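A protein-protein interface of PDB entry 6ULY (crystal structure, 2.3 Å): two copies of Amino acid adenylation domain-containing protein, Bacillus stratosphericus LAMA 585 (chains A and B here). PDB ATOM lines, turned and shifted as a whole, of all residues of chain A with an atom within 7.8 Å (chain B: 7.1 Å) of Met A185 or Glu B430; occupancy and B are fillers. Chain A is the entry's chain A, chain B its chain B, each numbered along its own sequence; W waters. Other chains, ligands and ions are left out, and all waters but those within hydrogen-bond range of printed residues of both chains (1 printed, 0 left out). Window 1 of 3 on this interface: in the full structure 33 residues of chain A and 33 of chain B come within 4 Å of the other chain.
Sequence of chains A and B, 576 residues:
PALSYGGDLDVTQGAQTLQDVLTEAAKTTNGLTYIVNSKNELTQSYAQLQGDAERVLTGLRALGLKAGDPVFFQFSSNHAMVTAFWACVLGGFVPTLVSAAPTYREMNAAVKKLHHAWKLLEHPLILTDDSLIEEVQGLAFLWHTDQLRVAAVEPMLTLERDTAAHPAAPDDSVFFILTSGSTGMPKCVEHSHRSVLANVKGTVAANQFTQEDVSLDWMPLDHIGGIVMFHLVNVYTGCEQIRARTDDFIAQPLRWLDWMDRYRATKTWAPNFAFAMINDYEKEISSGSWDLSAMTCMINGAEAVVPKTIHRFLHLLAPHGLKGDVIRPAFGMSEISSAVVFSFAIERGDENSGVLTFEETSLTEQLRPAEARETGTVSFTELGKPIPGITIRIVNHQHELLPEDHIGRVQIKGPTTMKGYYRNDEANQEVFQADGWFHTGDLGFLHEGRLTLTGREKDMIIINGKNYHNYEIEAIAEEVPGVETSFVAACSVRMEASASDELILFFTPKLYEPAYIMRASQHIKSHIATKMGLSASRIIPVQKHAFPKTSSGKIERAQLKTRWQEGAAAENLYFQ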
ATOM      1  N   MET A 107     -29.404   3.676  21.736  1.00  0.00           N
ATOM      2  CA  MET A 107     -27.990   3.340  21.895  1.00  0.00           C
ATOM      3  C   MET A 107     -27.306   3.307  20.528  1.00  0.00           C
ATOM      4  O   MET A 107     -26.889   2.264  20.020  1.00  0.00           O
ATOM      5  CB  MET A 107     -27.850   2.007  22.619  1.00  0.00           C
ATOM      6  CG  MET A 107     -26.445   1.696  23.102  1.00  0.00           C
ATOM      7  SD  MET A 107     -26.000   2.637  24.572  1.00  0.00           S
ATOM      8  CE  MET A 107     -24.318   2.075  24.845  1.00  0.00           C
ATOM      9  N   ALA A 109     -24.364   4.898  17.622  1.00  0.00           N
ATOM     10  CA  ALA A 109     -22.904   4.914  17.608  1.00  0.00           C
ATOM     11  C   ALA A 109     -22.353   6.041  18.471  1.00  0.00           C
ATOM     12  O   ALA A 109     -21.475   5.822  19.314  1.00  0.00           O
ATOM     13  CB  ALA A 109     -22.400   5.047  16.172  1.00  0.00           C
ATOM     14  N   ALA A 110     -22.842   7.264  18.257  1.00  0.00           N
ATOM     15  CA  ALA A 110     -22.370   8.395  19.048  1.00  0.00           C
ATOM     16  C   ALA A 110     -22.524   8.123  20.538  1.00  0.00           C
ATOM     17  O   ALA A 110     -21.622   8.420  21.328  1.00  0.00           O
ATOM     18  CB  ALA A 110     -23.127   9.664  18.652  1.00  0.00           C
ATOM     19  N   VAL A 111     -23.655   7.546  20.937  1.00  0.00           N
ATOM     20  CA  VAL A 111     -23.894   7.281  22.352  1.00  0.00           C
ATOM     21  C   VAL A 111     -22.926   6.226  22.873  1.00  0.00           C
ATOM     22  O   VAL A 111     -22.479   6.293  24.026  1.00  0.00           O
ATOM     23  CB  VAL A 111     -25.360   6.865  22.567  1.00  0.00           C
ATOM     24  CG1 VAL A 111     -25.551   6.267  23.951  1.00  0.00           C
ATOM     25  CG2 VAL A 111     -26.275   8.063  22.369  1.00  0.00           C
ATOM     26  N   LYS A 112     -22.593   5.232  22.045  1.00  0.00           N
ATOM     27  CA  LYS A 112     -21.615   4.227  22.452  1.00  0.00           C
ATOM     28  C   LYS A 112     -20.249   4.861  22.684  1.00  0.00           C
ATOM     29  O   LYS A 112     -19.575   4.571  23.679  1.00  0.00           O
ATOM     30  CB  LYS A 112     -21.515   3.124  21.393  1.00  0.00           C
ATOM     31  CG  LYS A 112     -22.765   2.273  21.237  1.00  0.00           C
ATOM     32  CD  LYS A 112     -22.547   1.131  20.250  1.00  0.00           C
ATOM     33  CE  LYS A 112     -23.798   0.273  20.101  1.00  0.00           C
ATOM     34  NZ  LYS A 112     -23.609  -0.837  19.124  1.00  0.00           N
ATOM     35  N   LYS A 113     -19.820   5.727  21.766  1.00  0.00           N
ATOM     36  CA  LYS A 113     -18.523   6.379  21.913  1.00  0.00           C
ATOM     37  C   LYS A 113     -18.472   7.238  23.173  1.00  0.00           C
ATOM     38  O   LYS A 113     -17.458   7.248  23.883  1.00  0.00           O
ATOM     39  CB  LYS A 113     -18.222   7.220  20.672  1.00  0.00           C
ATOM     40  CG  LYS A 113     -18.238   6.417  19.373  1.00  0.00           C
ATOM     41  CD  LYS A 113     -17.818   7.253  18.174  1.00  0.00           C
ATOM     42  CE  LYS A 113     -17.714   6.399  16.922  1.00  0.00           C
ATOM     43  NZ  LYS A 113     -17.015   7.105  15.811  1.00  0.00           N
ATOM     44  N   LEU A 114     -19.551   7.970  23.469  1.00  0.00           N
ATOM     45  CA  LEU A 114     -19.581   8.757  24.698  1.00  0.00           C
ATOM     46  C   LEU A 114     -19.406   7.863  25.918  1.00  0.00           C
ATOM     47  O   LEU A 114     -18.664   8.204  26.847  1.00  0.00           O
ATOM     48  CB  LEU A 114     -20.891   9.546  24.798  1.00  0.00           C
ATOM     49  CG  LEU A 114     -21.116  10.611  23.724  1.00  0.00           C
ATOM     50  CD1 LEU A 114     -22.510  11.210  23.842  1.00  0.00           C
ATOM     51  CD2 LEU A 114     -20.053  11.697  23.806  1.00  0.00           C
ATOM     52  N   HIS A 115     -20.076   6.708  25.928  1.00  0.00           N
ATOM     53  CA  HIS A 115     -19.951   5.794  27.058  1.00  0.00           C
ATOM     54  C   HIS A 115     -18.513   5.325  27.232  1.00  0.00           C
ATOM     55  O   HIS A 115     -18.023   5.204  28.361  1.00  0.00           O
ATOM     56  CB  HIS A 115     -20.873   4.590  26.871  1.00  0.00           C
ATOM     57  CG  HIS A 115     -20.750   3.567  27.958  1.00  0.00           C
ATOM     58  ND1 HIS A 115     -19.804   2.564  27.936  1.00  0.00           N
ATOM     59  CD2 HIS A 115     -21.450   3.399  29.105  1.00  0.00           C
ATOM     60  CE1 HIS A 115     -19.930   1.820  29.020  1.00  0.00           C
ATOM     61  NE2 HIS A 115     -20.922   2.305  29.746  1.00  0.00           N
ATOM     62  N   HIS A 116     -17.826   5.041  26.125  1.00  0.00           N
ATOM     63  CA  HIS A 116     -16.444   4.583  26.214  1.00  0.00           C
ATOM     64  C   HIS A 116     -15.574   5.626  26.903  1.00  0.00           C
ATOM     65  O   HIS A 116     -14.910   5.338  27.905  1.00  0.00           O
ATOM     66  CB  HIS A 116     -15.900   4.266  24.820  1.00  0.00           C
ATOM     67  CG  HIS A 116     -14.435   3.957  24.806  1.00  0.00           C
ATOM     68  ND1 HIS A 116     -13.939   2.694  25.049  1.00  0.00           N
ATOM     69  CD2 HIS A 116     -13.359   4.750  24.595  1.00  0.00           C
ATOM     70  CE1 HIS A 116     -12.620   2.719  24.979  1.00  0.00           C
ATOM     71  NE2 HIS A 116     -12.243   3.955  24.705  1.00  0.00           N
ATOM     72  N   ALA A 117     -15.559   6.849  26.366  1.00  0.00           N
ATOM     73  CA  ALA A 117     -14.760   7.911  26.971  1.00  0.00           C
ATOM     74  C   ALA A 117     -15.196   8.179  28.405  1.00  0.00           C
ATOM     75  O   ALA A 117     -14.358   8.371  29.293  1.00  0.00           O
ATOM     76  CB  ALA A 117     -14.865   9.187  26.138  1.00  0.00           C
ATOM     77  N   LYS A 119     -16.518   6.152  30.586  1.00  0.00           N
ATOM     78  CA  LYS A 119     -15.990   5.090  31.436  1.00  0.00           C
ATOM     79  C   LYS A 119     -14.471   5.163  31.542  1.00  0.00           C
ATOM     80  O   LYS A 119     -13.903   4.889  32.606  1.00  0.00           O
ATOM     81  CB  LYS A 119     -16.425   3.727  30.891  1.00  0.00           C
ATOM     82  CG  LYS A 119     -16.020   2.544  31.753  1.00  0.00           C
ATOM     83  CD  LYS A 119     -16.644   1.247  31.240  1.00  0.00           C
ATOM     84  CE  LYS A 119     -16.220   0.042  32.079  1.00  0.00           C
ATOM     85  NZ  LYS A 119     -16.839  -1.234  31.601  1.00  0.00           N
ATOM     86  N   LEU A 120     -13.791   5.517  30.449  1.00  0.00           N
ATOM     87  CA  LEU A 120     -12.337   5.632  30.499  1.00  0.00           C
ATOM     88  C   LEU A 120     -11.902   6.702  31.491  1.00  0.00           C
ATOM     89  O   LEU A 120     -10.854   6.567  32.132  1.00  0.00           O
ATOM     90  CB  LEU A 120     -11.789   5.948  29.106  1.00  0.00           C
ATOM     91  CG  LEU A 120     -10.270   5.849  28.956  1.00  0.00           C
ATOM     92  CD1 LEU A 120      -9.798   4.425  29.251  1.00  0.00           C
ATOM     93  CD2 LEU A 120      -9.829   6.294  27.565  1.00  0.00           C
ATOM     94  N   LEU A 178     -11.565  14.349  21.967  1.00  0.00           N
ATOM     95  CA  LEU A 178     -11.785  13.046  21.365  1.00  0.00           C
ATOM     96  C   LEU A 178     -11.568  13.107  19.861  1.00  0.00           C
ATOM     97  O   LEU A 178     -11.911  14.096  19.209  1.00  0.00           O
ATOM     98  CB  LEU A 178     -13.197  12.556  21.684  1.00  0.00           C
ATOM     99  CG  LEU A 178     -13.331  11.695  22.944  1.00  0.00           C
ATOM    100  CD1 LEU A 178     -12.515  12.223  24.114  1.00  0.00           C
ATOM    101  CD2 LEU A 178     -14.797  11.600  23.336  1.00  0.00           C
ATOM    102  N   THR A 179     -10.985  12.040  19.319  1.00  0.00           N
ATOM    103  CA  THR A 179     -10.673  11.968  17.897  1.00  0.00           C
ATOM    104  C   THR A 179     -11.923  11.719  17.064  1.00  0.00           C
ATOM    105  O   THR A 179     -12.857  11.057  17.518  1.00  0.00           O
ATOM    106  CB  THR A 179      -9.654  10.854  17.611  1.00  0.00           C
ATOM    107  OG1 THR A 179     -10.141   9.613  18.138  1.00  0.00           O
ATOM    108  CG2 THR A 179      -8.313  11.182  18.246  1.00  0.00           C
ATOM    109  N   GLY A 184     -14.156   3.073  14.687  1.00  0.00           N
ATOM    110  CA  GLY A 184     -13.716   2.552  15.969  1.00  0.00           C
ATOM    111  C   GLY A 184     -14.007   3.509  17.110  1.00  0.00           C
ATOM    112  O   GLY A 184     -14.518   4.609  16.893  1.00  0.00           O
ATOM    113  N   MET A 185     -13.688   3.088  18.329  1.00  0.00           N
ATOM    114  CA  MET A 185     -13.893   3.956  19.478  1.00  0.00           C
ATOM    115  C   MET A 185     -12.908   5.121  19.426  1.00  0.00           C
ATOM    116  O   MET A 185     -11.738   4.932  19.075  1.00  0.00           O
ATOM    117  CB  MET A 185     -13.717   3.183  20.787  1.00  0.00           C
ATOM    118  CG  MET A 185     -14.866   2.234  21.122  1.00  0.00           C
ATOM    119  SD  MET A 185     -16.467   3.061  21.257  1.00  0.00           S
ATOM    120  CE  MET A 185     -17.449   1.785  22.044  1.00  0.00           C
ATOM    121  N   PRO A 186     -13.342   6.333  19.766  1.00  0.00           N
ATOM    122  CA  PRO A 186     -12.422   7.473  19.726  1.00  0.00           C
ATOM    123  C   PRO A 186     -11.392   7.383  20.838  1.00  0.00           C
ATOM    124  O   PRO A 186     -11.627   6.787  21.893  1.00  0.00           O
ATOM    125  CB  PRO A 186     -13.344   8.684  19.909  1.00  0.00           C
ATOM    126  CG  PRO A 186     -14.500   8.157  20.698  1.00  0.00           C
ATOM    127  CD  PRO A 186     -14.676   6.714  20.270  1.00  0.00           C
ATOM    128  N   LYS A 187     -10.232   7.974  20.582  1.00  0.00           N
ATOM    129  CA  LYS A 187      -9.182   8.079  21.580  1.00  0.00           C
ATOM    130  C   LYS A 187      -9.255   9.440  22.263  1.00  0.00           C
ATOM    131  O   LYS A 187      -9.913  10.374  21.797  1.00  0.00           O
ATOM    132  CB  LYS A 187      -7.804   7.861  20.947  1.00  0.00           C
ATOM    133  CG  LYS A 187      -7.691   6.557  20.177  1.00  0.00           C
ATOM    134  CD  LYS A 187      -6.460   5.778  20.577  1.00  0.00           C
ATOM    135  CE  LYS A 187      -6.267   4.545  19.690  1.00  0.00           C
ATOM    136  NZ  LYS A 187      -7.365   3.544  19.831  1.00  0.00           N
ATOM    137  N   CYS A 188      -8.551   9.546  23.378  1.00  0.00           N
ATOM    138  CA  CYS A 188      -8.682  10.666  24.296  1.00  0.00           C
ATOM    139  C   CYS A 188      -7.385  11.470  24.283  1.00  0.00           C
ATOM    140  O   CYS A 188      -6.462  11.207  25.058  1.00  0.00           O
ATOM    141  CB  CYS A 188      -9.009  10.143  25.675  1.00  0.00           C
ATOM    142  SG  CYS A 188      -9.966  11.263  26.674  1.00  0.00           S
ATOM    143  N   ASN A 424      -3.775   4.680  27.283  1.00  0.00           N
ATOM    144  CA  ASN A 424      -3.532   3.788  26.150  1.00  0.00           C
ATOM    145  C   ASN A 424      -2.056   3.890  25.749  1.00  0.00           C
ATOM    146  O   ASN A 424      -1.693   4.490  24.736  1.00  0.00           O
ATOM    147  CB  ASN A 424      -4.450   4.111  24.974  1.00  0.00           C
ATOM    148  CG  ASN A 424      -4.427   3.029  23.922  1.00  0.00           C
ATOM    149  OD1 ASN A 424      -3.457   2.282  23.815  1.00  0.00           O
ATOM    150  ND2 ASN A 424      -5.497   2.931  23.144  1.00  0.00           N
ATOM    151  N   LYS B 187      -2.725  -7.102  19.595  1.00  0.00           N
ATOM    152  CA  LYS B 187      -2.641  -6.832  21.019  1.00  0.00           C
ATOM    153  C   LYS B 187      -1.957  -7.994  21.725  1.00  0.00           C
ATOM    154  O   LYS B 187      -1.871  -9.112  21.211  1.00  0.00           O
ATOM    155  CB  LYS B 187      -4.031  -6.573  21.601  1.00  0.00           C
ATOM    156  CG  LYS B 187      -4.717  -5.393  20.925  1.00  0.00           C
ATOM    157  CD  LYS B 187      -5.900  -4.876  21.700  1.00  0.00           C
ATOM    158  CE  LYS B 187      -6.729  -3.937  20.830  1.00  0.00           C
ATOM    159  NZ  LYS B 187      -5.883  -2.992  20.036  1.00  0.00           N
ATOM    160  N   HIS B 399     -26.679  -4.603  26.135  1.00  0.00           N
ATOM    161  CA  HIS B 399     -26.100  -5.570  27.067  1.00  0.00           C
ATOM    162  C   HIS B 399     -27.154  -6.167  27.994  1.00  0.00           C
ATOM    163  O   HIS B 399     -26.855  -6.559  29.127  1.00  0.00           O
ATOM    164  CB  HIS B 399     -24.962  -4.945  27.878  1.00  0.00           C
ATOM    165  CG  HIS B 399     -23.782  -4.547  27.046  1.00  0.00           C
ATOM    166  ND1 HIS B 399     -23.726  -4.761  25.685  1.00  0.00           N
ATOM    167  CD2 HIS B 399     -22.615  -3.949  27.381  1.00  0.00           C
ATOM    168  CE1 HIS B 399     -22.575  -4.310  25.218  1.00  0.00           C
ATOM    169  NE2 HIS B 399     -21.883  -3.813  26.226  1.00  0.00           N
ATOM    170  N   TYR B 421      -5.114  -7.058  27.968  1.00  0.00           N
ATOM    171  CA  TYR B 421      -4.164  -6.656  26.941  1.00  0.00           C
ATOM    172  C   TYR B 421      -3.053  -5.842  27.586  1.00  0.00           C
ATOM    173  O   TYR B 421      -3.310  -4.907  28.354  1.00  0.00           O
ATOM    174  CB  TYR B 421      -4.856  -5.843  25.845  1.00  0.00           C
ATOM    175  CG  TYR B 421      -5.995  -6.568  25.156  1.00  0.00           C
ATOM    176  CD1 TYR B 421      -5.778  -7.753  24.461  1.00  0.00           C
ATOM    177  CD2 TYR B 421      -7.288  -6.058  25.190  1.00  0.00           C
ATOM    178  CE1 TYR B 421      -6.820  -8.413  23.827  1.00  0.00           C
ATOM    179  CE2 TYR B 421      -8.332  -6.713  24.558  1.00  0.00           C
ATOM    180  CZ  TYR B 421      -8.093  -7.890  23.883  1.00  0.00           C
ATOM    181  OH  TYR B 421      -9.130  -8.537  23.255  1.00  0.00           O
ATOM    182  N   ASN B 424      -2.547  -1.588  27.781  1.00  0.00           N
ATOM    183  CA  ASN B 424      -3.633  -0.963  27.032  1.00  0.00           C
ATOM    184  C   ASN B 424      -4.888  -0.953  27.913  1.00  0.00           C
ATOM    185  O   ASN B 424      -5.806  -1.761  27.753  1.00  0.00           O
ATOM    186  CB  ASN B 424      -3.880  -1.677  25.705  1.00  0.00           C
ATOM    187  CG  ASN B 424      -4.777  -0.877  24.781  1.00  0.00           C
ATOM    188  OD1 ASN B 424      -5.567  -0.051  25.235  1.00  0.00           O
ATOM    189  ND2 ASN B 424      -4.656  -1.112  23.482  1.00  0.00           N
ATOM    190  N   ASP B 425      -4.928   0.005  28.847  1.00  0.00           N
ATOM    191  CA  ASP B 425      -6.115   0.183  29.683  1.00  0.00           C
ATOM    192  C   ASP B 425      -7.368   0.337  28.835  1.00  0.00           C
ATOM    193  O   ASP B 425      -8.417  -0.242  29.143  1.00  0.00           O
ATOM    194  CB  ASP B 425      -5.956   1.412  30.582  1.00  0.00           C
ATOM    195  CG  ASP B 425      -5.068   1.158  31.783  1.00  0.00           C
ATOM    196  OD1 ASP B 425      -4.459   0.071  31.870  1.00  0.00           O
ATOM    197  OD2 ASP B 425      -4.987   2.061  32.644  1.00  0.00           O
ATOM    198  N   GLU B 426      -7.274   1.112  27.755  1.00  0.00           N
ATOM    199  CA  GLU B 426      -8.455   1.437  26.963  1.00  0.00           C
ATOM    200  C   GLU B 426      -9.060   0.190  26.334  1.00  0.00           C
ATOM    201  O   GLU B 426     -10.271  -0.045  26.438  1.00  0.00           O
ATOM    202  CB  GLU B 426      -8.087   2.463  25.890  1.00  0.00           C
ATOM    203  CG  GLU B 426      -9.267   2.957  25.089  1.00  0.00           C
ATOM    204  CD  GLU B 426      -8.932   4.148  24.213  1.00  0.00           C
ATOM    205  OE1 GLU B 426      -7.738   4.511  24.116  1.00  0.00           O
ATOM    206  OE2 GLU B 426      -9.870   4.719  23.618  1.00  0.00           O
ATOM    207  N   ALA B 427      -8.234  -0.620  25.664  1.00  0.00           N
ATOM    208  CA  ALA B 427      -8.751  -1.838  25.045  1.00  0.00           C
ATOM    209  C   ALA B 427      -9.283  -2.808  26.090  1.00  0.00           C
ATOM    210  O   ALA B 427     -10.208  -3.575  25.809  1.00  0.00           O
ATOM    211  CB  ALA B 427      -7.663  -2.509  24.206  1.00  0.00           C
ATOM    212  N   ASN B 428      -8.712  -2.796  27.296  1.00  0.00           N
ATOM    213  CA  ASN B 428      -9.192  -3.692  28.343  1.00  0.00           C
ATOM    214  C   ASN B 428     -10.577  -3.286  28.833  1.00  0.00           C
ATOM    215  O   ASN B 428     -11.388  -4.150  29.183  1.00  0.00           O
ATOM    216  CB  ASN B 428      -8.188  -3.724  29.497  1.00  0.00           C
ATOM    217  CG  ASN B 428      -6.994  -4.618  29.198  1.00  0.00           C
ATOM    218  OD1 ASN B 428      -7.138  -5.658  28.562  1.00  0.00           O
ATOM    219  ND2 ASN B 428      -5.813  -4.214  29.648  1.00  0.00           N
ATOM    220  N   GLN B 429     -10.868  -1.986  28.858  1.00  0.00           N
ATOM    221  CA  GLN B 429     -12.220  -1.538  29.173  1.00  0.00           C
ATOM    222  C   GLN B 429     -13.224  -2.024  28.134  1.00  0.00           C
ATOM    223  O   GLN B 429     -14.330  -2.453  28.481  1.00  0.00           O
ATOM    224  CB  GLN B 429     -12.241  -0.016  29.262  1.00  0.00           C
ATOM    225  CG  GLN B 429     -13.620   0.596  29.246  1.00  0.00           C
ATOM    226  CD  GLN B 429     -13.557   2.105  29.293  1.00  0.00           C
ATOM    227  OE1 GLN B 429     -12.888   2.678  30.151  1.00  0.00           O
ATOM    228  NE2 GLN B 429     -14.232   2.754  28.354  1.00  0.00           N
ATOM    229  N   GLU B 430     -12.854  -1.964  26.853  1.00  0.00           N
ATOM    230  CA  GLU B 430     -13.793  -2.311  25.792  1.00  0.00           C
ATOM    231  C   GLU B 430     -14.265  -3.753  25.905  1.00  0.00           C
ATOM    232  O   GLU B 430     -15.422  -4.058  25.595  1.00  0.00           O
ATOM    233  CB  GLU B 430     -13.148  -2.075  24.426  1.00  0.00           C
ATOM    234  CG  GLU B 430     -12.933  -0.605  24.071  1.00  0.00           C
ATOM    235  CD  GLU B 430     -12.120  -0.427  22.796  1.00  0.00           C
ATOM    236  OE1 GLU B 430     -11.502  -1.410  22.341  1.00  0.00           O
ATOM    237  OE2 GLU B 430     -12.093   0.696  22.248  1.00  0.00           O
ATOM    238  N   VAL B 431     -13.385  -4.657  26.338  1.00  0.00           N
ATOM    239  CA  VAL B 431     -13.711  -6.079  26.346  1.00  0.00           C
ATOM    240  C   VAL B 431     -14.162  -6.519  27.733  1.00  0.00           C
ATOM    241  O   VAL B 431     -14.981  -7.435  27.861  1.00  0.00           O
ATOM    242  CB  VAL B 431     -12.517  -6.928  25.862  1.00  0.00           C
ATOM    243  CG1 VAL B 431     -12.175  -6.580  24.421  1.00  0.00           C
ATOM    244  CG2 VAL B 431     -11.302  -6.740  26.770  1.00  0.00           C
ATOM    245  N   PHE B 432     -13.637  -5.884  28.780  1.00  0.00           N
ATOM    246  CA  PHE B 432     -14.017  -6.228  30.151  1.00  0.00           C
ATOM    247  C   PHE B 432     -15.259  -5.427  30.524  1.00  0.00           C
ATOM    248  O   PHE B 432     -15.178  -4.293  31.000  1.00  0.00           O
ATOM    249  CB  PHE B 432     -12.868  -5.971  31.117  1.00  0.00           C
ATOM    250  CG  PHE B 432     -11.726  -6.946  30.987  1.00  0.00           C
ATOM    251  CD1 PHE B 432     -11.963  -8.293  30.780  1.00  0.00           C
ATOM    252  CD2 PHE B 432     -10.415  -6.509  31.072  1.00  0.00           C
ATOM    253  CE1 PHE B 432     -10.913  -9.187  30.658  1.00  0.00           C
ATOM    254  CE2 PHE B 432      -9.362  -7.396  30.954  1.00  0.00           C
ATOM    255  CZ  PHE B 432      -9.612  -8.737  30.747  1.00  0.00           C
ATOM    256  N   GLN B 433     -16.426  -6.031  30.309  1.00  0.00           N
ATOM    257  CA  GLN B 433     -17.694  -5.383  30.606  1.00  0.00           C
ATOM    258  C   GLN B 433     -18.035  -5.545  32.086  1.00  0.00           C
ATOM    259  O   GLN B 433     -17.328  -6.210  32.850  1.00  0.00           O
ATOM    260  CB  GLN B 433     -18.808  -5.961  29.730  1.00  0.00           C
ATOM    261  CG  GLN B 433     -18.553  -5.868  28.229  1.00  0.00           C
ATOM    262  CD  GLN B 433     -18.594  -4.444  27.710  1.00  0.00           C
ATOM    263  OE1 GLN B 433     -19.342  -3.604  28.215  1.00  0.00           O
ATOM    264  NE2 GLN B 433     -17.785  -4.162  26.695  1.00  0.00           N
ATOM    265  N   TRP B 437     -18.044  -9.852  32.696  1.00  0.00           N
ATOM    266  CA  TRP B 437     -18.294 -10.443  31.389  1.00  0.00           C
ATOM    267  C   TRP B 437     -17.272  -9.944  30.377  1.00  0.00           C
ATOM    268  O   TRP B 437     -16.977  -8.748  30.313  1.00  0.00           O
ATOM    269  CB  TRP B 437     -19.710 -10.122  30.902  1.00  0.00           C
ATOM    270  CG  TRP B 437     -20.764 -10.845  31.683  1.00  0.00           C
ATOM    271  CD1 TRP B 437     -21.512 -10.340  32.700  1.00  0.00           C
ATOM    272  CD2 TRP B 437     -21.175 -12.209  31.519  1.00  0.00           C
ATOM    273  NE1 TRP B 437     -22.369 -11.302  33.184  1.00  0.00           N
ATOM    274  CE2 TRP B 437     -22.181 -12.458  32.474  1.00  0.00           C
ATOM    275  CE3 TRP B 437     -20.794 -13.241  30.656  1.00  0.00           C
ATOM    276  CZ2 TRP B 437     -22.808 -13.696  32.593  1.00  0.00           C
ATOM    277  CZ3 TRP B 437     -21.419 -14.470  30.774  1.00  0.00           C
ATOM    278  CH2 TRP B 437     -22.414 -14.687  31.736  1.00  0.00           C
ATOM    279  N   PHE B 438     -16.739 -10.871  29.585  1.00  0.00           N
ATOM    280  CA  PHE B 438     -15.792 -10.552  28.527  1.00  0.00           C
ATOM    281  C   PHE B 438     -16.540 -10.461  27.201  1.00  0.00           C
ATOM    282  O   PHE B 438     -17.298 -11.369  26.849  1.00  0.00           O
ATOM    283  CB  PHE B 438     -14.682 -11.605  28.449  1.00  0.00           C
ATOM    284  CG  PHE B 438     -13.763 -11.416  27.281  1.00  0.00           C
ATOM    285  CD1 PHE B 438     -12.683 -10.554  27.361  1.00  0.00           C
ATOM    286  CD2 PHE B 438     -13.992 -12.085  26.093  1.00  0.00           C
ATOM    287  CE1 PHE B 438     -11.842 -10.372  26.278  1.00  0.00           C
ATOM    288  CE2 PHE B 438     -13.160 -11.903  25.009  1.00  0.00           C
ATOM    289  CZ  PHE B 438     -12.087 -11.043  25.100  1.00  0.00           C
ATOM    290  N   HIS B 439     -16.327  -9.366  26.475  1.00  0.00           N
ATOM    291  CA  HIS B 439     -16.999  -9.122  25.202  1.00  0.00           C
ATOM    292  C   HIS B 439     -16.167  -9.742  24.085  1.00  0.00           C
ATOM    293  O   HIS B 439     -15.074  -9.258  23.772  1.00  0.00           O
ATOM    294  CB  HIS B 439     -17.192  -7.625  24.972  1.00  0.00           C
ATOM    295  CG  HIS B 439     -18.307  -7.295  24.026  1.00  0.00           C
ATOM    296  ND1 HIS B 439     -19.630  -7.547  24.322  1.00  0.00           N
ATOM    297  CD2 HIS B 439     -18.298  -6.728  22.796  1.00  0.00           C
ATOM    298  CE1 HIS B 439     -20.388  -7.151  23.314  1.00  0.00           C
ATOM    299  NE2 HIS B 439     -19.604  -6.651  22.376  1.00  0.00           N
HETATM  300  O   HOH W   1      -7.340   7.285  24.840  1.00  0.00           O
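NE2 of His A116 lies within hydrogen-bond range of OE2 of Glu B426 (2.7 Å).
O of His A116 is in hydrogen-bond range of NE2 of Gln B429, at 2.7 Å.
The backbone carbonyl oxygen of Lys A119 lies close to the side-chain amide oxygen of Gln B429.
N of Leu A120 sits at hydrogen-bond distance from OE1 of Gln B429 (3.0 Å).
The side-chain amide oxygen of Asn A424 sits close to the side-chain amide oxygen of Asn B424.
OE1 of Glu B426 sits at hydrogen-bond distance from ND2 of Asn A424 (2.9 Å).
O of Pro A186 sits close to OE2 of Glu B426 (3.2 Å).
Asn B424 touches its own counterpart, Asn A424.
2 positions are printed for both chains.
Of the 12 pairs that touch across the chains among the printed residues, 1 has its exchanged pair printed and touching as well.
The side-chain hydroxyl (OG1) of Thr A179 is in hydrogen-bond range of the backbone NH (N) of Lys A187, 2.9 Å away.
The backbone NH (N) of Glu B426 lies close to the side-chain amide oxygen (OD1) of Asn B424.
OD1 of Asn B424 is in hydrogen-bond range of N of Ala B427, at 2.8 Å.
ND2 of Asn B428 sits at hydrogen-bond distance from O of Asn B424 (3.1 Å).
The backbone carbonyl oxygen (O) of Glu B430 lies within hydrogen-bond range of the side-chain amide nitrogen (NE2) of Gln B433, 2.6 Å away.
Among the printed residues, pairs that only touch across the chains: Met A185 with Glu B430, His A116 with Glu B430, Lys A119 with Phe B432, Lys A187 with Glu B426 and Leu A120 with Glu B426.
Water W1 lies within hydrogen-bond range of the side-chain carboxylate of Glu B426 (2.9 Å) and the backbone NH of Cys A188 (3.0 Å).
Of the 20 printed residues of chain A, 7 touch a printed residue of chain B.
Printed residues of chain B that touch a printed residue of chain A: Asn B424, Glu B426, Gln B429, Glu B430 and Phe B432.
Among the printed residues, 12 pairs touch across the chains.
Met A185 touches just one residue of chain B: Glu B430.
Glu B430 touches two residues of chain A.
Printed residues of chain A within 4 Å of Glu B426: His A116 (2.7 Å), Leu A120 (3.996 Å), Pro A186 (3.2 Å), Lys A187 (3.97 Å) and Asn A424 (2.9 Å).
Of the printed residues of chain B, Lys A187 touches Glu B426.
Of the printed residues of chain B, Lys A119 touches Gln B429 (3.3 Å) and Phe B432 (3.5 Å).
Of the printed residues of chain B, Leu A120 touches Glu B426 (3.996 Å) and Gln B429 (3.0 Å).
Gly A184 touches none of the printed residues of chain B.
The nearest residue of chain A that does not touch Glu B430 is Lys A187 (6.0 Å).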
